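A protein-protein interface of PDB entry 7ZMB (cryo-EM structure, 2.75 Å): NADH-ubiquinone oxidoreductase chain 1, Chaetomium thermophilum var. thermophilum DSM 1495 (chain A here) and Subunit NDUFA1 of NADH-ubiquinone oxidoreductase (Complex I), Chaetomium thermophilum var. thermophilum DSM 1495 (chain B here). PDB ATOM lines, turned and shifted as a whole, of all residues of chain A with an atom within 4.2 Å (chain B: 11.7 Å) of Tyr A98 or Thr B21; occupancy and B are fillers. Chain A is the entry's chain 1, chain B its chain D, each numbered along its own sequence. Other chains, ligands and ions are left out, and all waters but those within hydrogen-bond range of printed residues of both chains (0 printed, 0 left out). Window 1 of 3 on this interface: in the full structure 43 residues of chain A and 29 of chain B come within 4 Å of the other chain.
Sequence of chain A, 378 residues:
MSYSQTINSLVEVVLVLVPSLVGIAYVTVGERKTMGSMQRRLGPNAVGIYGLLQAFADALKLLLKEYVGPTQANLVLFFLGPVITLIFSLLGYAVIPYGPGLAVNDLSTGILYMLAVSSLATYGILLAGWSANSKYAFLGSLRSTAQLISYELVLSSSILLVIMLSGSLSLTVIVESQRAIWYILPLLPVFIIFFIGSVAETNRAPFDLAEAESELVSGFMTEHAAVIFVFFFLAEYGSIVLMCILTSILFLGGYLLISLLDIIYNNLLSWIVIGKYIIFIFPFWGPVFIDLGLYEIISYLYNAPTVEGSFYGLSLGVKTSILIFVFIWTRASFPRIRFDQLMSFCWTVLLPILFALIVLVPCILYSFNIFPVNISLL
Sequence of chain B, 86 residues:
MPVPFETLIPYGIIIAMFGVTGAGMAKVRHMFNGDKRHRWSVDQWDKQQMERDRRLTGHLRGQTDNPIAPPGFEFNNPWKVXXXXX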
ATOM      1  N   LEU A  15     -14.187  29.339   8.715  1.00  0.00           N
ATOM      2  CA  LEU A  15     -13.669  28.479   9.773  1.00  0.00           C
ATOM      3  C   LEU A  15     -14.664  28.266  10.903  1.00  0.00           C
ATOM      4  O   LEU A  15     -14.500  27.328  11.684  1.00  0.00           O
ATOM      5  CB  LEU A  15     -12.385  29.065  10.346  1.00  0.00           C
ATOM      6  CG  LEU A  15     -11.129  29.009   9.485  1.00  0.00           C
ATOM      7  CD1 LEU A  15     -10.153  30.080   9.933  1.00  0.00           C
ATOM      8  CD2 LEU A  15     -10.499  27.647   9.555  1.00  0.00           C
ATOM      9  N   PRO A  19     -16.907  24.128   9.735  1.00  0.00           N
ATOM     10  CA  PRO A  19     -16.752  23.088  10.757  1.00  0.00           C
ATOM     11  C   PRO A  19     -17.966  22.910  11.650  1.00  0.00           C
ATOM     12  O   PRO A  19     -18.189  21.790  12.121  1.00  0.00           O
ATOM     13  CB  PRO A  19     -15.532  23.561  11.550  1.00  0.00           C
ATOM     14  CG  PRO A  19     -14.756  24.302  10.559  1.00  0.00           C
ATOM     15  CD  PRO A  19     -15.787  25.078   9.813  1.00  0.00           C
ATOM     16  N   SER A  20     -18.760  23.950  11.894  1.00  0.00           N
ATOM     17  CA  SER A  20     -19.977  23.740  12.668  1.00  0.00           C
ATOM     18  C   SER A  20     -21.026  22.958  11.888  1.00  0.00           C
ATOM     19  O   SER A  20     -21.621  22.024  12.430  1.00  0.00           O
ATOM     20  CB  SER A  20     -20.562  25.073  13.139  1.00  0.00           C
ATOM     21  OG  SER A  20     -19.620  25.810  13.893  1.00  0.00           O
ATOM     22  N   TYR A  93     -23.844  31.182  16.605  1.00  0.00           N
ATOM     23  CA  TYR A  93     -22.447  30.777  16.552  1.00  0.00           C
ATOM     24  C   TYR A  93     -21.507  31.934  16.275  1.00  0.00           C
ATOM     25  O   TYR A  93     -20.295  31.715  16.211  1.00  0.00           O
ATOM     26  CB  TYR A  93     -22.240  29.700  15.485  1.00  0.00           C
ATOM     27  CG  TYR A  93     -22.886  28.374  15.811  1.00  0.00           C
ATOM     28  CD1 TYR A  93     -24.258  28.212  15.729  1.00  0.00           C
ATOM     29  CD2 TYR A  93     -22.123  27.289  16.201  1.00  0.00           C
ATOM     30  CE1 TYR A  93     -24.847  27.008  16.030  1.00  0.00           C
ATOM     31  CE2 TYR A  93     -22.704  26.079  16.504  1.00  0.00           C
ATOM     32  CZ  TYR A  93     -24.065  25.940  16.416  1.00  0.00           C
ATOM     33  OH  TYR A  93     -24.650  24.739  16.713  1.00  0.00           O
ATOM     34  N   ILE A  96     -19.390  32.803  19.770  1.00  0.00           N
ATOM     35  CA  ILE A  96     -18.746  31.749  20.547  1.00  0.00           C
ATOM     36  C   ILE A  96     -17.243  31.993  20.561  1.00  0.00           C
ATOM     37  O   ILE A  96     -16.626  32.079  19.493  1.00  0.00           O
ATOM     38  CB  ILE A  96     -19.079  30.362  19.980  1.00  0.00           C
ATOM     39  CG1 ILE A  96     -20.582  30.096  20.079  1.00  0.00           C
ATOM     40  CG2 ILE A  96     -18.249  29.283  20.664  1.00  0.00           C
ATOM     41  CD1 ILE A  96     -21.198  30.482  21.393  1.00  0.00           C
ATOM     42  N   PRO A  97     -16.613  32.126  21.728  1.00  0.00           N
ATOM     43  CA  PRO A  97     -15.146  32.209  21.762  1.00  0.00           C
ATOM     44  C   PRO A  97     -14.535  30.816  21.678  1.00  0.00           C
ATOM     45  O   PRO A  97     -14.783  29.965  22.533  1.00  0.00           O
ATOM     46  CB  PRO A  97     -14.853  32.867  23.115  1.00  0.00           C
ATOM     47  CG  PRO A  97     -16.117  32.886  23.871  1.00  0.00           C
ATOM     48  CD  PRO A  97     -17.235  32.385  23.036  1.00  0.00           C
ATOM     49  N   TYR A  98     -13.731  30.585  20.645  1.00  0.00           N
ATOM     50  CA  TYR A  98     -12.946  29.360  20.507  1.00  0.00           C
ATOM     51  C   TYR A  98     -11.530  29.578  21.011  1.00  0.00           C
ATOM     52  O   TYR A  98     -10.558  29.081  20.448  1.00  0.00           O
ATOM     53  CB  TYR A  98     -12.944  28.876  19.060  1.00  0.00           C
ATOM     54  CG  TYR A  98     -14.307  28.519  18.529  1.00  0.00           C
ATOM     55  CD1 TYR A  98     -15.140  29.491  17.998  1.00  0.00           C
ATOM     56  CD2 TYR A  98     -14.772  27.211  18.570  1.00  0.00           C
ATOM     57  CE1 TYR A  98     -16.387  29.176  17.515  1.00  0.00           C
ATOM     58  CE2 TYR A  98     -16.026  26.885  18.087  1.00  0.00           C
ATOM     59  CZ  TYR A  98     -16.826  27.872  17.559  1.00  0.00           C
ATOM     60  OH  TYR A  98     -18.075  27.582  17.071  1.00  0.00           O
ATOM     61  N   GLY A  99     -11.421  30.346  22.085  1.00  0.00           N
ATOM     62  CA  GLY A  99     -10.180  30.875  22.582  1.00  0.00           C
ATOM     63  C   GLY A  99     -10.473  32.266  23.083  1.00  0.00           C
ATOM     64  O   GLY A  99     -11.583  32.769  22.908  1.00  0.00           O
ATOM     65  N   LEU A 102     -11.509  34.709  20.443  1.00  0.00           N
ATOM     66  CA  LEU A 102     -11.485  34.067  19.129  1.00  0.00           C
ATOM     67  C   LEU A 102     -12.914  33.780  18.674  1.00  0.00           C
ATOM     68  O   LEU A 102     -13.356  32.639  18.543  1.00  0.00           O
ATOM     69  CB  LEU A 102     -10.648  32.798  19.173  1.00  0.00           C
ATOM     70  CG  LEU A 102      -9.145  33.013  19.214  1.00  0.00           C
ATOM     71  CD1 LEU A 102      -8.434  31.690  19.059  1.00  0.00           C
ATOM     72  CD2 LEU A 102      -8.738  33.977  18.122  1.00  0.00           C
ATOM     73  N   TYR A 312      -7.316  24.953  22.951  1.00  0.00           N
ATOM     74  CA  TYR A 312      -8.571  25.608  23.301  1.00  0.00           C
ATOM     75  C   TYR A 312      -9.738  25.008  22.524  1.00  0.00           C
ATOM     76  O   TYR A 312     -10.796  24.732  23.095  1.00  0.00           O
ATOM     77  CB  TYR A 312      -8.472  27.109  23.034  1.00  0.00           C
ATOM     78  CG  TYR A 312      -7.706  27.887  24.074  1.00  0.00           C
ATOM     79  CD1 TYR A 312      -7.727  27.516  25.408  1.00  0.00           C
ATOM     80  CD2 TYR A 312      -6.958  28.992  23.719  1.00  0.00           C
ATOM     81  CE1 TYR A 312      -7.032  28.230  26.353  1.00  0.00           C
ATOM     82  CE2 TYR A 312      -6.257  29.707  24.654  1.00  0.00           C
ATOM     83  CZ  TYR A 312      -6.297  29.332  25.965  1.00  0.00           C
ATOM     84  OH  TYR A 312      -5.590  30.061  26.887  1.00  0.00           O
ATOM     85  N   LEU A 316     -12.877  23.017  24.372  1.00  0.00           N
ATOM     86  CA  LEU A 316     -14.276  23.401  24.243  1.00  0.00           C
ATOM     87  C   LEU A 316     -15.096  22.278  23.623  1.00  0.00           C
ATOM     88  O   LEU A 316     -16.192  21.960  24.097  1.00  0.00           O
ATOM     89  CB  LEU A 316     -14.392  24.677  23.414  1.00  0.00           C
ATOM     90  CG  LEU A 316     -15.801  25.261  23.307  1.00  0.00           C
ATOM     91  CD1 LEU A 316     -16.395  25.472  24.679  1.00  0.00           C
ATOM     92  CD2 LEU A 316     -15.792  26.552  22.527  1.00  0.00           C
ATOM     93  N   GLY B  12     -15.642  11.855  18.109  1.00  0.00           N
ATOM     94  CA  GLY B  12     -14.290  12.264  17.766  1.00  0.00           C
ATOM     95  C   GLY B  12     -14.257  13.271  16.633  1.00  0.00           C
ATOM     96  O   GLY B  12     -13.407  14.164  16.609  1.00  0.00           O
ATOM     97  N   ILE B  13     -15.179  13.136  15.676  1.00  0.00           N
ATOM     98  CA  ILE B  13     -15.250  14.076  14.561  1.00  0.00           C
ATOM     99  C   ILE B  13     -15.780  15.427  15.026  1.00  0.00           C
ATOM    100  O   ILE B  13     -15.309  16.478  14.580  1.00  0.00           O
ATOM    101  CB  ILE B  13     -16.099  13.484  13.421  1.00  0.00           C
ATOM    102  CG1 ILE B  13     -15.315  12.391  12.687  1.00  0.00           C
ATOM    103  CG2 ILE B  13     -16.529  14.566  12.441  1.00  0.00           C
ATOM    104  CD1 ILE B  13     -16.123  11.656  11.664  1.00  0.00           C
ATOM    105  N   ILE B  14     -16.771  15.425  15.917  1.00  0.00           N
ATOM    106  CA  ILE B  14     -17.292  16.676  16.450  1.00  0.00           C
ATOM    107  C   ILE B  14     -16.200  17.430  17.193  1.00  0.00           C
ATOM    108  O   ILE B  14     -16.046  18.647  17.032  1.00  0.00           O
ATOM    109  CB  ILE B  14     -18.511  16.405  17.350  1.00  0.00           C
ATOM    110  CG1 ILE B  14     -19.645  15.787  16.541  1.00  0.00           C
ATOM    111  CG2 ILE B  14     -19.002  17.696  17.989  1.00  0.00           C
ATOM    112  CD1 ILE B  14     -20.754  15.255  17.382  1.00  0.00           C
ATOM    113  N   ILE B  15     -15.415  16.717  18.004  1.00  0.00           N
ATOM    114  CA  ILE B  15     -14.336  17.343  18.760  1.00  0.00           C
ATOM    115  C   ILE B  15     -13.282  17.910  17.816  1.00  0.00           C
ATOM    116  O   ILE B  15     -12.788  19.026  18.013  1.00  0.00           O
ATOM    117  CB  ILE B  15     -13.731  16.333  19.754  1.00  0.00           C
ATOM    118  CG1 ILE B  15     -14.612  16.228  20.994  1.00  0.00           C
ATOM    119  CG2 ILE B  15     -12.325  16.727  20.142  1.00  0.00           C
ATOM    120  CD1 ILE B  15     -14.471  14.946  21.742  1.00  0.00           C
ATOM    121  N   ALA B  16     -12.933  17.159  16.772  1.00  0.00           N
ATOM    122  CA  ALA B  16     -11.917  17.620  15.838  1.00  0.00           C
ATOM    123  C   ALA B  16     -12.337  18.897  15.126  1.00  0.00           C
ATOM    124  O   ALA B  16     -11.502  19.773  14.887  1.00  0.00           O
ATOM    125  CB  ALA B  16     -11.604  16.526  14.821  1.00  0.00           C
ATOM    126  N   MET B  17     -13.616  19.020  14.771  1.00  0.00           N
ATOM    127  CA  MET B  17     -14.080  20.229  14.099  1.00  0.00           C
ATOM    128  C   MET B  17     -13.938  21.454  14.988  1.00  0.00           C
ATOM    129  O   MET B  17     -13.592  22.535  14.500  1.00  0.00           O
ATOM    130  CB  MET B  17     -15.533  20.067  13.659  1.00  0.00           C
ATOM    131  CG  MET B  17     -15.779  19.010  12.604  1.00  0.00           C
ATOM    132  SD  MET B  17     -14.912  19.353  11.071  1.00  0.00           S
ATOM    133  CE  MET B  17     -13.542  18.213  11.217  1.00  0.00           C
ATOM    134  N   PHE B  18     -14.222  21.312  16.284  1.00  0.00           N
ATOM    135  CA  PHE B  18     -13.920  22.382  17.226  1.00  0.00           C
ATOM    136  C   PHE B  18     -12.427  22.656  17.291  1.00  0.00           C
ATOM    137  O   PHE B  18     -12.014  23.811  17.422  1.00  0.00           O
ATOM    138  CB  PHE B  18     -14.448  22.025  18.611  1.00  0.00           C
ATOM    139  CG  PHE B  18     -15.894  22.329  18.809  1.00  0.00           C
ATOM    140  CD1 PHE B  18     -16.295  23.560  19.270  1.00  0.00           C
ATOM    141  CD2 PHE B  18     -16.854  21.374  18.554  1.00  0.00           C
ATOM    142  CE1 PHE B  18     -17.627  23.837  19.454  1.00  0.00           C
ATOM    143  CE2 PHE B  18     -18.182  21.647  18.742  1.00  0.00           C
ATOM    144  CZ  PHE B  18     -18.569  22.875  19.188  1.00  0.00           C
ATOM    145  N   GLY B  19     -11.605  21.607  17.214  1.00  0.00           N
ATOM    146  CA  GLY B  19     -10.170  21.806  17.177  1.00  0.00           C
ATOM    147  C   GLY B  19      -9.713  22.509  15.916  1.00  0.00           C
ATOM    148  O   GLY B  19      -8.801  23.336  15.953  1.00  0.00           O
ATOM    149  N   VAL B  20     -10.335  22.183  14.785  1.00  0.00           N
ATOM    150  CA  VAL B  20     -10.032  22.857  13.529  1.00  0.00           C
ATOM    151  C   VAL B  20     -10.385  24.333  13.618  1.00  0.00           C
ATOM    152  O   VAL B  20      -9.647  25.194  13.128  1.00  0.00           O
ATOM    153  CB  VAL B  20     -10.773  22.164  12.371  1.00  0.00           C
ATOM    154  CG1 VAL B  20     -10.885  23.079  11.164  1.00  0.00           C
ATOM    155  CG2 VAL B  20     -10.071  20.875  12.005  1.00  0.00           C
ATOM    156  N   THR B  21     -11.520  24.646  14.241  1.00  0.00           N
ATOM    157  CA  THR B  21     -11.960  26.033  14.330  1.00  0.00           C
ATOM    158  C   THR B  21     -11.062  26.841  15.255  1.00  0.00           C
ATOM    159  O   THR B  21     -10.675  27.964  14.920  1.00  0.00           O
ATOM    160  CB  THR B  21     -13.415  26.079  14.789  1.00  0.00           C
ATOM    161  OG1 THR B  21     -14.238  25.520  13.764  1.00  0.00           O
ATOM    162  CG2 THR B  21     -13.869  27.507  15.070  1.00  0.00           C
ATOM    163  N   GLY B  22     -10.706  26.280  16.411  1.00  0.00           N
ATOM    164  CA  GLY B  22      -9.800  26.973  17.311  1.00  0.00           C
ATOM    165  C   GLY B  22      -8.418  27.154  16.719  1.00  0.00           C
ATOM    166  O   GLY B  22      -7.793  28.202  16.884  1.00  0.00           O
ATOM    167  N   ALA B  23      -7.918  26.130  16.027  1.00  0.00           N
ATOM    168  CA  ALA B  23      -6.631  26.250  15.355  1.00  0.00           C
ATOM    169  C   ALA B  23      -6.692  27.260  14.221  1.00  0.00           C
ATOM    170  O   ALA B  23      -5.756  28.039  14.028  1.00  0.00           O
ATOM    171  CB  ALA B  23      -6.189  24.889  14.833  1.00  0.00           C
ATOM    172  N   GLY B  24      -7.783  27.260  13.458  1.00  0.00           N
ATOM    173  CA  GLY B  24      -7.875  28.162  12.320  1.00  0.00           C
ATOM    174  C   GLY B  24      -7.985  29.619  12.724  1.00  0.00           C
ATOM    175  O   GLY B  24      -7.286  30.476  12.181  1.00  0.00           O
ATOM    176  N   MET B  25      -8.864  29.919  13.683  1.00  0.00           N
ATOM    177  CA  MET B  25      -9.060  31.298  14.119  1.00  0.00           C
ATOM    178  C   MET B  25      -7.761  31.902  14.631  1.00  0.00           C
ATOM    179  O   MET B  25      -7.411  33.038  14.292  1.00  0.00           O
ATOM    180  CB  MET B  25     -10.129  31.360  15.212  1.00  0.00           C
ATOM    181  CG  MET B  25     -11.539  30.986  14.797  1.00  0.00           C
ATOM    182  SD  MET B  25     -12.222  32.056  13.524  1.00  0.00           S
ATOM    183  CE  MET B  25     -12.427  33.567  14.445  1.00  0.00           C
ATOM    184  N   ALA B  26      -7.031  31.152  15.451  1.00  0.00           N
ATOM    185  CA  ALA B  26      -5.827  31.689  16.069  1.00  0.00           C
ATOM    186  C   ALA B  26      -4.744  31.971  15.035  1.00  0.00           C
ATOM    187  O   ALA B  26      -4.062  32.996  15.111  1.00  0.00           O
ATOM    188  CB  ALA B  26      -5.324  30.725  17.139  1.00  0.00           C
ATOM    189  N   LYS B  27      -4.570  31.080  14.063  1.00  0.00           N
ATOM    190  CA  LYS B  27      -3.513  31.273  13.076  1.00  0.00           C
ATOM    191  C   LYS B  27      -3.790  32.482  12.190  1.00  0.00           C
ATOM    192  O   LYS B  27      -2.888  33.282  11.924  1.00  0.00           O
ATOM    193  CB  LYS B  27      -3.351  30.003  12.239  1.00  0.00           C
ATOM    194  CG  LYS B  27      -2.361  30.115  11.103  1.00  0.00           C
ATOM    195  CD  LYS B  27      -0.942  30.158  11.613  1.00  0.00           C
ATOM    196  CE  LYS B  27       0.028  30.562  10.525  1.00  0.00           C
ATOM    197  NZ  LYS B  27       1.403  30.768  11.059  1.00  0.00           N
ATOM    198  N   VAL B  28      -5.028  32.605  11.705  1.00  0.00           N
ATOM    199  CA  VAL B  28      -5.363  33.713  10.769  1.00  0.00           C
ATOM    200  C   VAL B  28      -5.330  35.067  11.483  1.00  0.00           C
ATOM    201  O   VAL B  28      -5.045  36.057  10.810  1.00  0.00           O
ATOM    202  CB  VAL B  28      -6.687  33.465  10.014  1.00  0.00           C
ATOM    203  CG1 VAL B  28      -6.679  32.128   9.294  1.00  0.00           C
ATOM    204  CG2 VAL B  28      -7.905  33.590  10.912  1.00  0.00           C
ATOM    205  N   ARG B  29      -5.598  35.107  12.785  1.00  0.00           N
ATOM    206  CA  ARG B  29      -5.520  36.405  13.488  1.00  0.00           C
ATOM    207  C   ARG B  29      -4.093  36.627  13.978  1.00  0.00           C
ATOM    208  O   ARG B  29      -3.739  37.786  14.176  1.00  0.00           O
ATOM    209  CB  ARG B  29      -6.641  36.602  14.523  1.00  0.00           C
ATOM    210  CG  ARG B  29      -7.862  37.305  13.958  1.00  0.00           C
ATOM    211  CD  ARG B  29      -8.535  38.374  14.794  1.00  0.00           C
ATOM    212  NE  ARG B  29      -8.857  37.982  16.157  1.00  0.00           N
ATOM    213  CZ  ARG B  29      -9.967  37.366  16.540  1.00  0.00           C
ATOM    214  NH1 ARG B  29     -10.139  37.074  17.814  1.00  0.00           N
ATOM    215  NH2 ARG B  29     -10.890  37.028  15.659  1.00  0.00           N
ATOM    216  N   HIS B  30      -3.311  35.556  14.123  1.00  0.00           N
ATOM    217  CA  HIS B  30      -1.897  35.716  14.548  1.00  0.00           C
ATOM    218  C   HIS B  30      -1.202  36.231  13.302  1.00  0.00           C
ATOM    219  O   HIS B  30      -0.345  37.099  13.439  1.00  0.00           O
ATOM    220  CB  HIS B  30      -1.333  34.422  15.146  1.00  0.00           C
ATOM    221  CG  HIS B  30       0.089  34.509  15.587  1.00  0.00           C
ATOM    222  ND1 HIS B  30       1.141  34.252  14.732  1.00  0.00           N
ATOM    223  CD2 HIS B  30       0.635  34.782  16.790  1.00  0.00           C
ATOM    224  CE1 HIS B  30       2.274  34.369  15.389  1.00  0.00           C
ATOM    225  NE2 HIS B  30       1.993  34.703  16.649  1.00  0.00           N
ATOM    226  N   ARG B  37       0.018  37.694  18.748  1.00  0.00           N
ATOM    227  CA  ARG B  37      -1.293  37.286  19.306  1.00  0.00           C
ATOM    228  C   ARG B  37      -2.216  38.501  19.239  1.00  0.00           C
ATOM    229  O   ARG B  37      -1.724  39.624  19.425  1.00  0.00           O
ATOM    230  CB  ARG B  37      -1.165  36.616  20.677  1.00  0.00           C
ATOM    231  CG  ARG B  37      -2.494  36.312  21.351  1.00  0.00           C
ATOM    232  CD  ARG B  37      -2.494  35.115  22.284  1.00  0.00           C
ATOM    233  NE  ARG B  37      -1.611  35.239  23.432  1.00  0.00           N
ATOM    234  CZ  ARG B  37      -0.491  34.545  23.606  1.00  0.00           C
ATOM    235  NH1 ARG B  37       0.244  34.737  24.688  1.00  0.00           N
ATOM    236  NH2 ARG B  37      -0.111  33.660  22.702  1.00  0.00           N
ATOM    237  N   HIS B  38      -3.487  38.281  18.940  1.00  0.00           N
ATOM    238  CA  HIS B  38      -4.477  39.374  18.768  1.00  0.00           C
ATOM    239  C   HIS B  38      -4.838  40.024  20.103  1.00  0.00           C
ATOM    240  O   HIS B  38      -4.253  39.657  21.116  1.00  0.00           O
ATOM    241  CB  HIS B  38      -5.707  38.749  18.125  1.00  0.00           C
ATOM    242  CG  HIS B  38      -6.349  37.739  19.017  1.00  0.00           C
ATOM    243  ND1 HIS B  38      -5.808  36.487  19.227  1.00  0.00           N
ATOM    244  CD2 HIS B  38      -7.455  37.804  19.786  1.00  0.00           C
ATOM    245  CE1 HIS B  38      -6.553  35.822  20.079  1.00  0.00           C
ATOM    246  NE2 HIS B  38      -7.573  36.606  20.427  1.00  0.00           N
ATOM    247  N   TRP B  40      -8.131  41.107  22.782  1.00  0.00           N
ATOM    248  CA  TRP B  40      -9.542  40.827  23.134  1.00  0.00           C
ATOM    249  C   TRP B  40      -9.970  41.714  24.301  1.00  0.00           C
ATOM    250  O   TRP B  40      -9.078  42.280  24.949  1.00  0.00           O
ATOM    251  CB  TRP B  40      -9.747  39.345  23.460  1.00  0.00           C
ATOM    252  CG  TRP B  40      -8.955  38.811  24.611  1.00  0.00           C
ATOM    253  CD1 TRP B  40      -9.353  38.730  25.912  1.00  0.00           C
ATOM    254  CD2 TRP B  40      -7.636  38.240  24.560  1.00  0.00           C
ATOM    255  NE1 TRP B  40      -8.369  38.167  26.675  1.00  0.00           N
ATOM    256  CE2 TRP B  40      -7.302  37.857  25.875  1.00  0.00           C
ATOM    257  CE3 TRP B  40      -6.702  38.030  23.541  1.00  0.00           C
ATOM    258  CZ2 TRP B  40      -6.078  37.271  26.194  1.00  0.00           C
ATOM    259  CZ3 TRP B  40      -5.494  37.449  23.855  1.00  0.00           C
ATOM    260  CH2 TRP B  40      -5.189  37.074  25.165  1.00  0.00           C
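O of Leu A15 lies within hydrogen-bond range of OG1 of Thr B21 (2.8 Å).
The side-chain hydroxyl (OG1) of Thr B21 lies within hydrogen-bond range of the backbone carbonyl oxygen (O) of Met B17.
Among the printed residues, merely in contact across the chains: Leu A15 with Gly B24, Leu A15 with Met B25, Pro A19 with Met B17, Pro A19 with Thr B21, Tyr A98 with Phe B18, Tyr A98 with Thr B21, Tyr A98 with Gly B22, Leu A102 with Ala B26, Leu A102 with Arg B29 and Leu A102 with His B38.
Of chain B, only Thr B21 (2.8 Å), Gly B24 (3.6 Å) and Met B25 (3.97 Å) come within 4 Å of Leu A15. Of chain B, only Met B17 and Thr B21 come within 4 Å of Pro A19. No residue of chain B comes within 4 Å of Tyr A93. No residue of chain B comes within 4 Å of Pro A97. Of chain B, only Phe B18, Thr B21 and Gly B22 come within 4 Å of Tyr A98. No residue of chain B comes within 4 Å of Gly A99. Of chain B, only Ala B26 (3.8 Å), Arg B29 (3.4 Å) and His B38 (3.5 Å) come within 4 Å of Leu A102. Of chain A, only Leu A15, Pro A19 and Tyr A98 come within 4 Å of Thr B21. Printed residues of chain A within 4 Å of Gly B22: Tyr A98. Printed residues of chain A within 4 Å of Gly B24: Leu A15. Of the printed residues of chain A, Ala B26 touches Leu A102 (3.8 Å). The nearest printed residue of chain A that does not touch Thr B21 is Ser A20 (5.1 Å).
Of the 22 printed residues of chain B, 9 touch a printed residue of chain A. Hydrophobic or aromatic side chains of chain B that line the printed part of chain A: Met B17, Phe B18, Ala B26 and His B38. Hydrophobic or aromatic side chains of chain A that line the printed part of chain B: Leu A15, Pro A19, Tyr A98 and Leu A102. Among the printed residues, 11 pairs touch across the chains. Among the printed residues, no Asp or Glu carboxylate lies within 4 Å of a Lys or Arg side-chain nitrogen of the other chain.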
